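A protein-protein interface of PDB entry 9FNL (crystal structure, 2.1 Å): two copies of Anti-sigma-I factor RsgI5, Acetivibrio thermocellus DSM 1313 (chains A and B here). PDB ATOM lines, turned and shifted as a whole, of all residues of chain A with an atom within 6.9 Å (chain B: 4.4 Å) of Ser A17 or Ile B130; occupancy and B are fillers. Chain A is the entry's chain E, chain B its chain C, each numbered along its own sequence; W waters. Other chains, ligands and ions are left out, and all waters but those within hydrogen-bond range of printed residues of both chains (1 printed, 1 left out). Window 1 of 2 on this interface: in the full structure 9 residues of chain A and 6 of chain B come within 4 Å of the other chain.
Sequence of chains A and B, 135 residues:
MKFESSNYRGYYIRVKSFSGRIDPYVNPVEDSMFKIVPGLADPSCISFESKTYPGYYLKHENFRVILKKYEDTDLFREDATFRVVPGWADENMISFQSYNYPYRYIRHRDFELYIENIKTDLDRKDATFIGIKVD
The backbone carbonyl oxygen of Phe A18 sits at hydrogen-bond distance from the guanidinium group of Arg B9 (2.7 Å).
The guanidinium group (NH2) of Arg B9 sits at hydrogen-bond distance from the backbone carbonyl oxygen (O) of Leu A67, 3.0 Å away.
O of Gly B131 lies within hydrogen-bond range of OG of Ser A17 (3.0 Å).
The backbone carbonyl oxygen (O) of Lys B2 is in hydrogen-bond range of the backbone NH (N) of Ile B132 (2.9 Å).
OE2 of Glu B4 lies within salt-bridge range of NE of Arg B9, 2.9 Å away.
The backbone carbonyl oxygen (O) of Glu B4 sits at hydrogen-bond distance from the backbone NH (N) of Ile B130 (2.8 Å).
N of Leu A67 is in hydrogen-bond range of O of Phe A18 (3.0 Å).
Ser A17 touches Ile B130 (O to CG2, 3.4 Å).
Ser A17 touches Ile B132.
Ser A17 touches just these residues of chain B: Ile B130 (3.4 Å), Gly B131 (3.0 Å) and Ile B132 (3.8 Å).
Printed residues of chain B within 4 Å of Phe A18: Arg B9.
Of the printed residues of chain B, Leu A67 touches Arg B9 (3.0 Å).
Phe B3 touches none of the printed residues of chain A.
Of the printed residues of chain A, Ile B130 touches Ser A17.
Of the printed residues of chain A, Gly B131 touches Ser A17.
Of the printed residues of chain A, Ile B132 touches Ser A17 (3.8 Å).
The nearest printed residue of chain A that does not touch Ile B130 is Phe A18 (4.02 Å).
The nearest printed residue of chain B that does not touch Phe A18 is Ile B130 (4.02 Å).
Of the 10 printed residues of chain A, 3 touch a printed residue of chain B.
Printed residues of chain A that touch a printed residue of chain B: Ser A17, Phe A18 and Leu A67.
Hydrophobic or aromatic side chains of chain A within 4 Å of the printed part of chain B: Phe A18.
Of the 9 printed residues of chain B, 4 touch a printed residue of chain A.
No position is printed for both chains.
Of the 5 pairs that touch across the chains among the printed residues, none has its exchanged pair printed and touching as well.
Water W1 lies within hydrogen-bond range of O of Gly B131 (2.8 Å) and OG of Ser A17 (3.3 Å).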
ATOM      1  N   ARG A  14      24.502 -26.006 -18.276  1.00  0.00           N
ATOM      2  CA  ARG A  14      25.069 -25.928 -16.938  1.00  0.00           C
ATOM      3  C   ARG A  14      24.129 -26.593 -15.946  1.00  0.00           C
ATOM      4  O   ARG A  14      22.933 -26.759 -16.199  1.00  0.00           O
ATOM      5  CB  ARG A  14      25.360 -24.472 -16.510  1.00  0.00           C
ATOM      6  CG  ARG A  14      24.130 -23.555 -16.356  1.00  0.00           C
ATOM      7  CD  ARG A  14      23.481 -23.598 -14.954  1.00  0.00           C
ATOM      8  NE  ARG A  14      24.389 -23.249 -13.860  1.00  0.00           N
ATOM      9  CZ  ARG A  14      24.673 -21.999 -13.495  1.00  0.00           C
ATOM     10  NH1 ARG A  14      24.130 -20.971 -14.140  1.00  0.00           N
ATOM     11  NH2 ARG A  14      25.506 -21.775 -12.492  1.00  0.00           N
ATOM     12  N   VAL A  15      24.686 -26.946 -14.796  1.00  0.00           N
ATOM     13  CA  VAL A  15      23.927 -27.543 -13.704  1.00  0.00           C
ATOM     14  C   VAL A  15      23.672 -26.474 -12.651  1.00  0.00           C
ATOM     15  O   VAL A  15      24.595 -25.763 -12.236  1.00  0.00           O
ATOM     16  CB  VAL A  15      24.668 -28.742 -13.097  1.00  0.00           C
ATOM     17  CG1 VAL A  15      23.952 -29.210 -11.821  1.00  0.00           C
ATOM     18  CG2 VAL A  15      24.766 -29.887 -14.125  1.00  0.00           C
ATOM     19  N   LYS A  16      22.416 -26.351 -12.237  1.00  0.00           N
ATOM     20  CA  LYS A  16      22.002 -25.417 -11.196  1.00  0.00           C
ATOM     21  C   LYS A  16      21.064 -26.182 -10.275  1.00  0.00           C
ATOM     22  O   LYS A  16      20.049 -26.704 -10.741  1.00  0.00           O
ATOM     23  CB  LYS A  16      21.319 -24.196 -11.823  1.00  0.00           C
ATOM     24  CG  LYS A  16      20.549 -23.302 -10.861  1.00  0.00           C
ATOM     25  CD  LYS A  16      21.451 -22.798  -9.763  1.00  0.00           C
ATOM     26  CE  LYS A  16      22.383 -21.726 -10.276  1.00  0.00           C
ATOM     27  NZ  LYS A  16      23.310 -21.263  -9.196  1.00  0.00           N
ATOM     28  N   SER A  17      21.420 -26.287  -8.992  1.00  0.00           N
ATOM     29  CA  SER A  17      20.664 -27.099  -8.028  1.00  0.00           C
ATOM     30  C   SER A  17      20.368 -28.489  -8.593  1.00  0.00           C
ATOM     31  O   SER A  17      19.246 -28.987  -8.511  1.00  0.00           O
ATOM     32  CB  SER A  17      19.359 -26.409  -7.601  1.00  0.00           C
ATOM     33  OG  SER A  17      19.606 -25.151  -7.009  1.00  0.00           O
ATOM     34  N   PHE A  18      21.377 -29.089  -9.228  1.00  0.00           N
ATOM     35  CA  PHE A  18      21.319 -30.456  -9.742  1.00  0.00           C
ATOM     36  C   PHE A  18      20.310 -30.626 -10.880  1.00  0.00           C
ATOM     37  O   PHE A  18      19.862 -31.746 -11.149  1.00  0.00           O
ATOM     38  CB  PHE A  18      21.039 -31.456  -8.611  1.00  0.00           C
ATOM     39  CG  PHE A  18      22.118 -31.488  -7.578  1.00  0.00           C
ATOM     40  CD1 PHE A  18      23.205 -32.332  -7.724  1.00  0.00           C
ATOM     41  CD2 PHE A  18      22.069 -30.643  -6.478  1.00  0.00           C
ATOM     42  CE1 PHE A  18      24.207 -32.352  -6.790  1.00  0.00           C
ATOM     43  CE2 PHE A  18      23.070 -30.658  -5.544  1.00  0.00           C
ATOM     44  CZ  PHE A  18      24.143 -31.510  -5.695  1.00  0.00           C
ATOM     45  N   SER A  19      19.949 -29.546 -11.567  1.00  0.00           N
ATOM     46  CA  SER A  19      19.096 -29.617 -12.748  1.00  0.00           C
ATOM     47  C   SER A  19      19.765 -28.943 -13.935  1.00  0.00           C
ATOM     48  O   SER A  19      20.488 -27.953 -13.785  1.00  0.00           O
ATOM     49  CB  SER A  19      17.737 -28.966 -12.511  1.00  0.00           C
ATOM     50  OG  SER A  19      16.817 -29.943 -12.098  1.00  0.00           O
ATOM     51  N   GLY A  20      19.486 -29.467 -15.129  1.00  0.00           N
ATOM     52  CA  GLY A  20      20.132 -28.983 -16.342  1.00  0.00           C
ATOM     53  C   GLY A  20      19.423 -27.776 -16.943  1.00  0.00           C
ATOM     54  O   GLY A  20      18.199 -27.740 -17.042  1.00  0.00           O
ATOM     55  N   ARG A  21      20.215 -26.789 -17.351  1.00  0.00           N
ATOM     56  CA  ARG A  21      19.675 -25.607 -17.995  1.00  0.00           C
ATOM     57  C   ARG A  21      20.761 -24.989 -18.868  1.00  0.00           C
ATOM     58  O   ARG A  21      21.903 -25.454 -18.890  1.00  0.00           O
ATOM     59  CB  ARG A  21      19.138 -24.610 -16.960  1.00  0.00           C
ATOM     60  CG  ARG A  21      20.070 -24.270 -15.801  1.00  0.00           C
ATOM     61  CD  ARG A  21      19.401 -23.262 -14.816  1.00  0.00           C
ATOM     62  NE  ARG A  21      18.948 -22.055 -15.505  1.00  0.00           N
ATOM     63  CZ  ARG A  21      17.675 -21.760 -15.768  1.00  0.00           C
ATOM     64  NH1 ARG A  21      16.693 -22.571 -15.371  1.00  0.00           N
ATOM     65  NH2 ARG A  21      17.384 -20.639 -16.420  1.00  0.00           N
ATOM     66  N   ASP A  31      30.219 -24.835 -13.274  1.00  0.00           N
ATOM     67  CA  ASP A  31      28.906 -25.439 -13.461  1.00  0.00           C
ATOM     68  C   ASP A  31      28.628 -25.807 -14.909  1.00  0.00           C
ATOM     69  O   ASP A  31      27.751 -26.639 -15.155  1.00  0.00           O
ATOM     70  CB  ASP A  31      27.808 -24.495 -12.987  1.00  0.00           C
ATOM     71  CG  ASP A  31      27.655 -24.483 -11.474  1.00  0.00           C
ATOM     72  OD1 ASP A  31      28.472 -25.140 -10.779  1.00  0.00           O
ATOM     73  OD2 ASP A  31      26.725 -23.798 -10.990  1.00  0.00           O
ATOM     74  N   LEU A  67      21.173 -33.711 -12.926  1.00  0.00           N
ATOM     75  CA  LEU A  67      22.431 -34.259 -12.447  1.00  0.00           C
ATOM     76  C   LEU A  67      22.131 -35.191 -11.288  1.00  0.00           C
ATOM     77  O   LEU A  67      21.402 -34.821 -10.363  1.00  0.00           O
ATOM     78  CB  LEU A  67      23.399 -33.158 -12.000  1.00  0.00           C
ATOM     79  CG  LEU A  67      24.815 -33.698 -11.758  1.00  0.00           C
ATOM     80  CD1 LEU A  67      25.474 -33.952 -13.097  1.00  0.00           C
ATOM     81  CD2 LEU A  67      25.666 -32.767 -10.911  1.00  0.00           C
ATOM     82  N   LYS B   2      12.186 -23.320  -3.103  1.00  0.00           N
ATOM     83  CA  LYS B   2      11.505 -24.600  -3.083  1.00  0.00           C
ATOM     84  C   LYS B   2      12.539 -25.671  -2.752  1.00  0.00           C
ATOM     85  O   LYS B   2      13.749 -25.421  -2.745  1.00  0.00           O
ATOM     86  CB  LYS B   2      10.795 -24.882  -4.419  1.00  0.00           C
ATOM     87  CG  LYS B   2      11.737 -25.103  -5.584  1.00  0.00           C
ATOM     88  CD  LYS B   2      11.232 -24.462  -6.879  1.00  0.00           C
ATOM     89  CE  LYS B   2       9.838 -24.943  -7.246  1.00  0.00           C
ATOM     90  NZ  LYS B   2       9.690 -25.128  -8.735  1.00  0.00           N
ATOM     91  N   PHE B   3      12.049 -26.868  -2.439  1.00  0.00           N
ATOM     92  CA  PHE B   3      12.901 -27.939  -1.943  1.00  0.00           C
ATOM     93  C   PHE B   3      12.490 -29.246  -2.598  1.00  0.00           C
ATOM     94  O   PHE B   3      11.356 -29.699  -2.424  1.00  0.00           O
ATOM     95  CB  PHE B   3      12.816 -28.006  -0.415  1.00  0.00           C
ATOM     96  CG  PHE B   3      13.294 -26.745   0.244  1.00  0.00           C
ATOM     97  CD1 PHE B   3      14.644 -26.557   0.498  1.00  0.00           C
ATOM     98  CD2 PHE B   3      12.409 -25.721   0.541  1.00  0.00           C
ATOM     99  CE1 PHE B   3      15.102 -25.375   1.078  1.00  0.00           C
ATOM    100  CE2 PHE B   3      12.854 -24.535   1.131  1.00  0.00           C
ATOM    101  CZ  PHE B   3      14.204 -24.361   1.392  1.00  0.00           C
ATOM    102  N   GLU B   4      13.401 -29.821  -3.375  1.00  0.00           N
ATOM    103  CA  GLU B   4      13.150 -31.029  -4.141  1.00  0.00           C
ATOM    104  C   GLU B   4      13.653 -32.240  -3.371  1.00  0.00           C
ATOM    105  O   GLU B   4      14.730 -32.201  -2.772  1.00  0.00           O
ATOM    106  CB  GLU B   4      13.850 -30.957  -5.508  1.00  0.00           C
ATOM    107  CG  GLU B   4      13.489 -32.084  -6.466  1.00  0.00           C
ATOM    108  CD  GLU B   4      14.244 -32.009  -7.798  1.00  0.00           C
ATOM    109  OE1 GLU B   4      14.866 -30.963  -8.080  1.00  0.00           O
ATOM    110  OE2 GLU B   4      14.216 -33.000  -8.566  1.00  0.00           O
ATOM    111  N   ARG B   9      13.081 -37.348  -7.314  1.00  0.00           N
ATOM    112  CA  ARG B   9      13.364 -36.142  -8.079  1.00  0.00           C
ATOM    113  C   ARG B   9      12.107 -35.678  -8.807  1.00  0.00           C
ATOM    114  O   ARG B   9      11.322 -36.491  -9.305  1.00  0.00           O
ATOM    115  CB  ARG B   9      14.500 -36.398  -9.077  1.00  0.00           C
ATOM    116  CG  ARG B   9      15.821 -36.782  -8.422  1.00  0.00           C
ATOM    117  CD  ARG B   9      16.370 -35.640  -7.570  1.00  0.00           C
ATOM    118  NE  ARG B   9      16.691 -34.487  -8.399  1.00  0.00           N
ATOM    119  CZ  ARG B   9      17.873 -34.280  -8.972  1.00  0.00           C
ATOM    120  NH1 ARG B   9      18.053 -33.214  -9.722  1.00  0.00           N
ATOM    121  NH2 ARG B   9      18.878 -35.131  -8.780  1.00  0.00           N
ATOM    122  N   MET B  93      23.983 -32.102  -0.718  1.00  0.00           N
ATOM    123  CA  MET B  93      22.593 -31.684  -0.572  1.00  0.00           C
ATOM    124  C   MET B  93      22.360 -31.291   0.890  1.00  0.00           C
ATOM    125  O   MET B  93      23.316 -31.105   1.654  1.00  0.00           O
ATOM    126  CB  MET B  93      21.658 -32.799  -1.063  1.00  0.00           C
ATOM    127  CG  MET B  93      21.826 -33.103  -2.562  1.00  0.00           C
ATOM    128  SD  MET B  93      20.921 -34.556  -3.128  1.00  0.00           S
ATOM    129  CE  MET B  93      21.388 -34.571  -4.870  1.00  0.00           C
ATOM    130  N   PHE B 129      17.318 -33.334   0.707  1.00  0.00           N
ATOM    131  CA  PHE B 129      16.585 -32.437  -0.166  1.00  0.00           C
ATOM    132  C   PHE B 129      17.564 -31.539  -0.912  1.00  0.00           C
ATOM    133  O   PHE B 129      18.729 -31.397  -0.527  1.00  0.00           O
ATOM    134  CB  PHE B 129      15.577 -31.571   0.629  1.00  0.00           C
ATOM    135  CG  PHE B 129      14.466 -32.369   1.286  1.00  0.00           C
ATOM    136  CD1 PHE B 129      13.310 -32.699   0.578  1.00  0.00           C
ATOM    137  CD2 PHE B 129      14.585 -32.795   2.603  1.00  0.00           C
ATOM    138  CE1 PHE B 129      12.302 -33.435   1.167  1.00  0.00           C
ATOM    139  CE2 PHE B 129      13.567 -33.536   3.213  1.00  0.00           C
ATOM    140  CZ  PHE B 129      12.425 -33.855   2.493  1.00  0.00           C
ATOM    141  N   ILE B 130      17.058 -30.922  -1.976  1.00  0.00           N
ATOM    142  CA  ILE B 130      17.808 -30.011  -2.838  1.00  0.00           C
ATOM    143  C   ILE B 130      17.158 -28.642  -2.716  1.00  0.00           C
ATOM    144  O   ILE B 130      15.974 -28.489  -3.032  1.00  0.00           O
ATOM    145  CB  ILE B 130      17.802 -30.479  -4.307  1.00  0.00           C
ATOM    146  CG1 ILE B 130      18.492 -31.838  -4.465  1.00  0.00           C
ATOM    147  CG2 ILE B 130      18.451 -29.430  -5.221  1.00  0.00           C
ATOM    148  CD1 ILE B 130      18.083 -32.582  -5.728  1.00  0.00           C
ATOM    149  N   GLY B 131      17.922 -27.651  -2.259  1.00  0.00           N
ATOM    150  CA  GLY B 131      17.415 -26.288  -2.212  1.00  0.00           C
ATOM    151  C   GLY B 131      17.462 -25.653  -3.593  1.00  0.00           C
ATOM    152  O   GLY B 131      18.466 -25.761  -4.306  1.00  0.00           O
ATOM    153  N   ILE B 132      16.368 -24.997  -3.982  1.00  0.00           N
ATOM    154  CA  ILE B 132      16.259 -24.366  -5.294  1.00  0.00           C
ATOM    155  C   ILE B 132      15.812 -22.928  -5.099  1.00  0.00           C
ATOM    156  O   ILE B 132      14.698 -22.682  -4.622  1.00  0.00           O
ATOM    157  CB  ILE B 132      15.270 -25.092  -6.218  1.00  0.00           C
ATOM    158  CG1 ILE B 132      15.699 -26.535  -6.473  1.00  0.00           C
ATOM    159  CG2 ILE B 132      15.122 -24.329  -7.531  1.00  0.00           C
ATOM    160  CD1 ILE B 132      14.565 -27.397  -6.982  1.00  0.00           C
HETATM  161  O   HOH W   1      21.037 -26.803  -4.584  1.00  0.00           O
